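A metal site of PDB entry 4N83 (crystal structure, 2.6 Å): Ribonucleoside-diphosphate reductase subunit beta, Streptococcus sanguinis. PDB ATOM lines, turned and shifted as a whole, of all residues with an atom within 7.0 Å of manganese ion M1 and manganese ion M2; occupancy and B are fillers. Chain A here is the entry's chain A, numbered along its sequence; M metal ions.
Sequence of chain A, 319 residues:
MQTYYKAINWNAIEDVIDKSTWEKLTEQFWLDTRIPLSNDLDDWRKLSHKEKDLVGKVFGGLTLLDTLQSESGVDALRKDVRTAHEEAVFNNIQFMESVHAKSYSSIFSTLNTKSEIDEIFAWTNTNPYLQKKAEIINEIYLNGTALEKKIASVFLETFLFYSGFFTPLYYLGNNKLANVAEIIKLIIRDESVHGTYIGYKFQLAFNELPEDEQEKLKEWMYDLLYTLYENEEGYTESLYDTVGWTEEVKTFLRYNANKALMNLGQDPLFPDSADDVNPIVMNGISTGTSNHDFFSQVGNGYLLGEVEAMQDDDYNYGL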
ATOM      1  N   LEU A  62     -11.896 -24.552 -19.101  1.00  0.00           N
ATOM      2  CA  LEU A  62     -12.153 -23.891 -20.376  1.00  0.00           C
ATOM      3  C   LEU A  62     -13.438 -23.045 -20.311  1.00  0.00           C
ATOM      4  O   LEU A  62     -13.523 -21.997 -20.951  1.00  0.00           O
ATOM      5  CB  LEU A  62     -12.284 -24.927 -21.494  1.00  0.00           C
ATOM      6  CG  LEU A  62     -11.054 -25.803 -21.781  1.00  0.00           C
ATOM      7  CD1 LEU A  62     -11.444 -26.972 -22.674  1.00  0.00           C
ATOM      8  CD2 LEU A  62      -9.931 -24.988 -22.393  1.00  0.00           C
ATOM      9  N   LEU A  65     -12.791 -19.569 -19.509  1.00  0.00           N
ATOM     10  CA  LEU A  65     -12.207 -18.778 -20.588  1.00  0.00           C
ATOM     11  C   LEU A  65     -13.172 -18.500 -21.749  1.00  0.00           C
ATOM     12  O   LEU A  65     -13.000 -17.515 -22.473  1.00  0.00           O
ATOM     13  CB  LEU A  65     -10.953 -19.457 -21.115  1.00  0.00           C
ATOM     14  CG  LEU A  65      -9.854 -19.704 -20.072  1.00  0.00           C
ATOM     15  CD1 LEU A  65      -8.783 -20.636 -20.632  1.00  0.00           C
ATOM     16  CD2 LEU A  65      -9.241 -18.397 -19.595  1.00  0.00           C
ATOM     17  N   ASP A  66     -14.176 -19.350 -21.932  1.00  0.00           N
ATOM     18  CA  ASP A  66     -15.262 -19.070 -22.875  1.00  0.00           C
ATOM     19  C   ASP A  66     -16.241 -18.057 -22.285  1.00  0.00           C
ATOM     20  O   ASP A  66     -16.938 -17.348 -23.028  1.00  0.00           O
ATOM     21  CB  ASP A  66     -15.996 -20.356 -23.309  1.00  0.00           C
ATOM     22  CG  ASP A  66     -15.406 -20.974 -24.569  1.00  0.00           C
ATOM     23  OD1 ASP A  66     -15.301 -20.277 -25.587  1.00  0.00           O
ATOM     24  OD2 ASP A  66     -15.067 -22.176 -24.532  1.00  0.00           O
ATOM     25  N   GLN A  69     -14.369 -14.671 -22.724  1.00  0.00           N
ATOM     26  CA  GLN A  69     -14.449 -14.179 -24.099  1.00  0.00           C
ATOM     27  C   GLN A  69     -15.821 -13.576 -24.430  1.00  0.00           C
ATOM     28  O   GLN A  69     -15.896 -12.503 -25.039  1.00  0.00           O
ATOM     29  CB  GLN A  69     -14.125 -15.294 -25.097  1.00  0.00           C
ATOM     30  CG  GLN A  69     -12.653 -15.686 -25.138  1.00  0.00           C
ATOM     31  CD  GLN A  69     -11.782 -14.666 -25.843  1.00  0.00           C
ATOM     32  OE1 GLN A  69     -11.426 -14.835 -26.999  1.00  0.00           O
ATOM     33  NE2 GLN A  69     -11.446 -13.595 -25.141  1.00  0.00           N
ATOM     34  N   VAL A  74     -14.636 -10.215 -26.486  1.00  0.00           N
ATOM     35  CA  VAL A  74     -15.054  -9.712 -27.804  1.00  0.00           C
ATOM     36  C   VAL A  74     -15.532  -8.264 -27.686  1.00  0.00           C
ATOM     37  O   VAL A  74     -15.452  -7.495 -28.647  1.00  0.00           O
ATOM     38  CB  VAL A  74     -16.150 -10.589 -28.434  1.00  0.00           C
ATOM     39  CG1 VAL A  74     -16.504 -10.076 -29.831  1.00  0.00           C
ATOM     40  CG2 VAL A  74     -15.701 -12.051 -28.509  1.00  0.00           C
ATOM     41  N   LEU A  77     -12.510  -6.241 -28.268  1.00  0.00           N
ATOM     42  CA  LEU A  77     -12.133  -6.324 -29.683  1.00  0.00           C
ATOM     43  C   LEU A  77     -13.044  -5.505 -30.592  1.00  0.00           C
ATOM     44  O   LEU A  77     -12.608  -5.027 -31.646  1.00  0.00           O
ATOM     45  CB  LEU A  77     -12.124  -7.787 -30.143  1.00  0.00           C
ATOM     46  CG  LEU A  77     -11.053  -8.687 -29.510  1.00  0.00           C
ATOM     47  CD1 LEU A  77     -11.389 -10.157 -29.714  1.00  0.00           C
ATOM     48  CD2 LEU A  77      -9.677  -8.368 -30.076  1.00  0.00           C
ATOM     49  N   ILE A  93     -19.436 -13.500 -33.480  1.00  0.00           N
ATOM     50  CA  ILE A  93     -18.356 -14.144 -32.728  1.00  0.00           C
ATOM     51  C   ILE A  93     -18.721 -14.204 -31.247  1.00  0.00           C
ATOM     52  O   ILE A  93     -18.616 -15.258 -30.630  1.00  0.00           O
ATOM     53  CB  ILE A  93     -17.009 -13.411 -32.898  1.00  0.00           C
ATOM     54  CG1 ILE A  93     -16.494 -13.569 -34.340  1.00  0.00           C
ATOM     55  CG2 ILE A  93     -15.973 -13.954 -31.917  1.00  0.00           C
ATOM     56  CD1 ILE A  93     -15.418 -12.582 -34.735  1.00  0.00           C
ATOM     57  N   MET A  96     -21.453 -16.758 -30.362  1.00  0.00           N
ATOM     58  CA  MET A  96     -20.929 -18.128 -30.413  1.00  0.00           C
ATOM     59  C   MET A  96     -20.012 -18.447 -29.234  1.00  0.00           C
ATOM     60  O   MET A  96     -19.935 -19.595 -28.810  1.00  0.00           O
ATOM     61  CB  MET A  96     -20.208 -18.395 -31.746  1.00  0.00           C
ATOM     62  CG  MET A  96     -21.116 -18.437 -32.965  1.00  0.00           C
ATOM     63  SD  MET A  96     -22.578 -19.482 -32.795  1.00  0.00           S
ATOM     64  CE  MET A  96     -21.843 -21.040 -32.283  1.00  0.00           C
ATOM     65  N   GLU A  97     -19.325 -17.433 -28.708  1.00  0.00           N
ATOM     66  CA  GLU A  97     -18.502 -17.606 -27.506  1.00  0.00           C
ATOM     67  C   GLU A  97     -19.369 -17.939 -26.288  1.00  0.00           C
ATOM     68  O   GLU A  97     -18.936 -18.681 -25.400  1.00  0.00           O
ATOM     69  CB  GLU A  97     -17.648 -16.366 -27.216  1.00  0.00           C
ATOM     70  CG  GLU A  97     -16.634 -16.007 -28.308  1.00  0.00           C
ATOM     71  CD  GLU A  97     -15.462 -16.968 -28.416  1.00  0.00           C
ATOM     72  OE1 GLU A  97     -15.479 -18.021 -27.742  1.00  0.00           O
ATOM     73  OE2 GLU A  97     -14.530 -16.676 -29.179  1.00  0.00           O
ATOM     74  N   SER A  98     -20.585 -17.400 -26.247  1.00  0.00           N
ATOM     75  CA  SER A  98     -21.557 -17.750 -25.198  1.00  0.00           C
ATOM     76  C   SER A  98     -22.107 -19.163 -25.377  1.00  0.00           C
ATOM     77  O   SER A  98     -22.376 -19.851 -24.389  1.00  0.00           O
ATOM     78  CB  SER A  98     -22.718 -16.742 -25.153  1.00  0.00           C
ATOM     79  OG  SER A  98     -22.400 -15.621 -24.340  1.00  0.00           O
ATOM     80  N   HIS A 100     -20.387 -21.598 -26.688  1.00  0.00           N
ATOM     81  CA  HIS A 100     -19.272 -22.428 -26.220  1.00  0.00           C
ATOM     82  C   HIS A 100     -19.277 -22.538 -24.706  1.00  0.00           C
ATOM     83  O   HIS A 100     -19.052 -23.616 -24.149  1.00  0.00           O
ATOM     84  CB  HIS A 100     -17.925 -21.853 -26.701  1.00  0.00           C
ATOM     85  CG  HIS A 100     -17.784 -21.763 -28.189  1.00  0.00           C
ATOM     86  ND1 HIS A 100     -16.792 -21.032 -28.800  1.00  0.00           N
ATOM     87  CD2 HIS A 100     -18.538 -22.279 -29.192  1.00  0.00           C
ATOM     88  CE1 HIS A 100     -16.918 -21.115 -30.111  1.00  0.00           C
ATOM     89  NE2 HIS A 100     -17.977 -21.874 -30.371  1.00  0.00           N
ATOM     90  N   ALA A 101     -19.536 -21.415 -24.030  1.00  0.00           N
ATOM     91  CA  ALA A 101     -19.596 -21.396 -22.573  1.00  0.00           C
ATOM     92  C   ALA A 101     -20.747 -22.244 -22.032  1.00  0.00           C
ATOM     93  O   ALA A 101     -20.591 -22.954 -21.038  1.00  0.00           O
ATOM     94  CB  ALA A 101     -19.729 -19.955 -22.077  1.00  0.00           C
ATOM     95  N   TYR A 104     -20.655 -26.555 -22.278  1.00  0.00           N
ATOM     96  CA  TYR A 104     -20.027 -27.299 -21.187  1.00  0.00           C
ATOM     97  C   TYR A 104     -21.043 -27.704 -20.119  1.00  0.00           C
ATOM     98  O   TYR A 104     -20.977 -28.799 -19.573  1.00  0.00           O
ATOM     99  CB  TYR A 104     -18.916 -26.481 -20.528  1.00  0.00           C
ATOM    100  CG  TYR A 104     -17.814 -26.051 -21.467  1.00  0.00           C
ATOM    101  CD1 TYR A 104     -17.041 -26.990 -22.150  1.00  0.00           C
ATOM    102  CD2 TYR A 104     -17.533 -24.707 -21.673  1.00  0.00           C
ATOM    103  CE1 TYR A 104     -16.030 -26.595 -23.013  1.00  0.00           C
ATOM    104  CE2 TYR A 104     -16.523 -24.298 -22.537  1.00  0.00           C
ATOM    105  CZ  TYR A 104     -15.772 -25.253 -23.200  1.00  0.00           C
ATOM    106  OH  TYR A 104     -14.765 -24.850 -24.052  1.00  0.00           O
ATOM    107  N   SER A 153      -6.255 -12.802 -27.626  1.00  0.00           N
ATOM    108  CA  SER A 153      -7.403 -13.634 -27.993  1.00  0.00           C
ATOM    109  C   SER A 153      -6.998 -14.793 -28.908  1.00  0.00           C
ATOM    110  O   SER A 153      -7.574 -15.884 -28.827  1.00  0.00           O
ATOM    111  CB  SER A 153      -8.488 -12.790 -28.666  1.00  0.00           C
ATOM    112  OG  SER A 153      -9.692 -13.529 -28.801  1.00  0.00           O
ATOM    113  N   GLU A 157      -7.389 -18.807 -27.512  1.00  0.00           N
ATOM    114  CA  GLU A 157      -8.250 -19.837 -28.084  1.00  0.00           C
ATOM    115  C   GLU A 157      -7.606 -20.724 -29.156  1.00  0.00           C
ATOM    116  O   GLU A 157      -8.110 -21.810 -29.438  1.00  0.00           O
ATOM    117  CB  GLU A 157      -9.530 -19.197 -28.620  1.00  0.00           C
ATOM    118  CG  GLU A 157     -10.297 -18.450 -27.541  1.00  0.00           C
ATOM    119  CD  GLU A 157     -11.600 -17.868 -28.047  1.00  0.00           C
ATOM    120  OE1 GLU A 157     -11.559 -17.005 -28.952  1.00  0.00           O
ATOM    121  OE2 GLU A 157     -12.665 -18.267 -27.530  1.00  0.00           O
ATOM    122  N   PHE A 161      -5.976 -22.978 -25.234  1.00  0.00           N
ATOM    123  CA  PHE A 161      -7.244 -23.702 -25.108  1.00  0.00           C
ATOM    124  C   PHE A 161      -7.023 -25.205 -25.333  1.00  0.00           C
ATOM    125  O   PHE A 161      -7.755 -26.033 -24.791  1.00  0.00           O
ATOM    126  CB  PHE A 161      -8.276 -23.191 -26.121  1.00  0.00           C
ATOM    127  CG  PHE A 161      -9.400 -22.391 -25.511  1.00  0.00           C
ATOM    128  CD1 PHE A 161     -10.723 -22.779 -25.683  1.00  0.00           C
ATOM    129  CD2 PHE A 161      -9.148 -21.244 -24.780  1.00  0.00           C
ATOM    130  CE1 PHE A 161     -11.761 -22.051 -25.133  1.00  0.00           C
ATOM    131  CE2 PHE A 161     -10.180 -20.501 -24.237  1.00  0.00           C
ATOM    132  CZ  PHE A 161     -11.495 -20.908 -24.402  1.00  0.00           C
ATOM    133  N   PHE A 165      -8.396 -29.271 -24.827  1.00  0.00           N
ATOM    134  CA  PHE A 165      -8.907 -30.058 -25.969  1.00  0.00           C
ATOM    135  C   PHE A 165      -8.199 -31.405 -26.156  1.00  0.00           C
ATOM    136  O   PHE A 165      -8.747 -32.301 -26.786  1.00  0.00           O
ATOM    137  CB  PHE A 165      -8.819 -29.255 -27.276  1.00  0.00           C
ATOM    138  CG  PHE A 165      -9.737 -28.058 -27.356  1.00  0.00           C
ATOM    139  CD1 PHE A 165     -11.027 -28.102 -26.832  1.00  0.00           C
ATOM    140  CD2 PHE A 165      -9.318 -26.891 -27.991  1.00  0.00           C
ATOM    141  CE1 PHE A 165     -11.869 -27.002 -26.923  1.00  0.00           C
ATOM    142  CE2 PHE A 165     -10.153 -25.790 -28.088  1.00  0.00           C
ATOM    143  CZ  PHE A 165     -11.432 -25.846 -27.551  1.00  0.00           C
ATOM    144  N   ILE A 187     -16.638 -26.599 -31.455  1.00  0.00           N
ATOM    145  CA  ILE A 187     -16.021 -25.414 -30.838  1.00  0.00           C
ATOM    146  C   ILE A 187     -14.690 -25.076 -31.509  1.00  0.00           C
ATOM    147  O   ILE A 187     -14.399 -23.900 -31.768  1.00  0.00           O
ATOM    148  CB  ILE A 187     -15.812 -25.600 -29.318  1.00  0.00           C
ATOM    149  CG1 ILE A 187     -17.168 -25.637 -28.600  1.00  0.00           C
ATOM    150  CG2 ILE A 187     -14.951 -24.490 -28.737  1.00  0.00           C
ATOM    151  CD1 ILE A 187     -17.126 -26.225 -27.203  1.00  0.00           C
ATOM    152  N   ASP A 190     -15.187 -23.431 -34.934  1.00  0.00           N
ATOM    153  CA  ASP A 190     -15.465 -21.996 -34.805  1.00  0.00           C
ATOM    154  C   ASP A 190     -14.212 -21.206 -34.438  1.00  0.00           C
ATOM    155  O   ASP A 190     -13.942 -20.165 -35.031  1.00  0.00           O
ATOM    156  CB  ASP A 190     -16.551 -21.731 -33.760  1.00  0.00           C
ATOM    157  CG  ASP A 190     -17.946 -22.053 -34.261  1.00  0.00           C
ATOM    158  OD1 ASP A 190     -18.200 -21.960 -35.475  1.00  0.00           O
ATOM    159  OD2 ASP A 190     -18.806 -22.412 -33.413  1.00  0.00           O
ATOM    160  N   GLU A 191     -13.459 -21.713 -33.473  1.00  0.00           N
ATOM    161  CA  GLU A 191     -12.270 -21.008 -32.985  1.00  0.00           C
ATOM    162  C   GLU A 191     -11.123 -21.023 -33.993  1.00  0.00           C
ATOM    163  O   GLU A 191     -10.275 -20.126 -33.988  1.00  0.00           O
ATOM    164  CB  GLU A 191     -11.800 -21.573 -31.640  1.00  0.00           C
ATOM    165  CG  GLU A 191     -12.767 -21.351 -30.479  1.00  0.00           C
ATOM    166  CD  GLU A 191     -13.110 -19.888 -30.252  1.00  0.00           C
ATOM    167  OE1 GLU A 191     -12.331 -18.999 -30.679  1.00  0.00           O
ATOM    168  OE2 GLU A 191     -14.163 -19.603 -29.652  1.00  0.00           O
ATOM    169  N   HIS A 194     -12.059 -18.047 -35.990  1.00  0.00           N
ATOM    170  CA  HIS A 194     -11.882 -16.819 -35.199  1.00  0.00           C
ATOM    171  C   HIS A 194     -10.417 -16.381 -35.182  1.00  0.00           C
ATOM    172  O   HIS A 194     -10.120 -15.210 -35.418  1.00  0.00           O
ATOM    173  CB  HIS A 194     -12.370 -17.016 -33.759  1.00  0.00           C
ATOM    174  CG  HIS A 194     -13.852 -17.149 -33.637  1.00  0.00           C
ATOM    175  ND1 HIS A 194     -14.458 -17.825 -32.591  1.00  0.00           N
ATOM    176  CD2 HIS A 194     -14.853 -16.690 -34.420  1.00  0.00           C
ATOM    177  CE1 HIS A 194     -15.765 -17.784 -32.748  1.00  0.00           C
ATOM    178  NE2 HIS A 194     -16.034 -17.094 -33.840  1.00  0.00           N
ATOM    179  N   GLY A 195      -9.530 -17.328 -34.905  1.00  0.00           N
ATOM    180  CA  GLY A 195      -8.094 -17.062 -34.910  1.00  0.00           C
ATOM    181  C   GLY A 195      -7.606 -16.516 -36.235  1.00  0.00           C
ATOM    182  O   GLY A 195      -6.836 -15.550 -36.275  1.00  0.00           O
ATOM    183  N   ILE A 198      -9.331 -12.823 -36.662  1.00  0.00           N
ATOM    184  CA  ILE A 198      -8.717 -11.875 -35.731  1.00  0.00           C
ATOM    185  C   ILE A 198      -7.232 -11.698 -36.072  1.00  0.00           C
ATOM    186  O   ILE A 198      -6.712 -10.576 -36.044  1.00  0.00           O
ATOM    187  CB  ILE A 198      -8.868 -12.335 -34.258  1.00  0.00           C
ATOM    188  CG1 ILE A 198     -10.344 -12.295 -33.835  1.00  0.00           C
ATOM    189  CG2 ILE A 198      -8.048 -11.443 -33.330  1.00  0.00           C
ATOM    190  CD1 ILE A 198     -10.645 -13.001 -32.530  1.00  0.00           C
HETATM  191 MN    MN M   1     -12.786 -16.625 -30.439  1.00  0.00          MN
HETATM  192 MN    MN M   2     -14.400 -19.945 -27.479  1.00  0.00          MN
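Merely in contact with manganese ion M1: His 194.
Within 4 Å of manganese ion M1: Glu 97, Glu 157, Glu 191 and His 194.
Within 4 Å of manganese ion M2: Asp 66, Glu 97, His 100, Glu 157 and Glu 191.
The side-chain carboxylate (OE1) of Glu 157 lies close to the side-chain amide oxygen (OE1) of Gln 69, 2.9 Å away.
The side-chain hydroxyl of Tyr 104 sits at hydrogen-bond distance from the side-chain carboxylate of Asp 66 (2.7 Å).
ND1 of His 100 sits close to OE1 of Glu 97.
OE2 of Glu 191 sits close to ND1 of His 100.
A ring nitrogen (ND1) of His 194 sits close to the side-chain carboxylate (OE1) of Glu 191 (3.1 Å).
A ring nitrogen (NE2) of His 100 lies close to the backbone carbonyl oxygen of Met 96 (3.4 Å).
The side-chain carboxylate of Asp 190 sits at hydrogen-bond distance from a ring nitrogen (NE2) of His 100 (3.2 Å).
ND1 of His 194 sits close to O of Asp 190, at 3.4 Å.
Manganese ion M1 is bound by OE1 of Glu 157 (2.0 Å).
OE2 of Glu 97 binds manganese ion M1.
Manganese ion M1 is bound by the side-chain carboxylate (OE1) of Glu 191, at 2.4 Å.
Manganese ion M1 has three donor atoms within binding distance.
Manganese ion M2 is bound by OD1 of Asp 66 (2.1 Å).
Manganese ion M2 is bound by OE2 of Glu 191.
The side-chain carboxylate (OE1) of Glu 97 is bound to manganese ion M2 (2.2 Å).
Manganese ion M2 is bound by OE2 of Glu 157 (2.4 Å).
Manganese ion M2 has four donor atoms within binding distance.
Slightly farther from manganese ion M2 lies ND1 of His 100 (2.9 Å).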
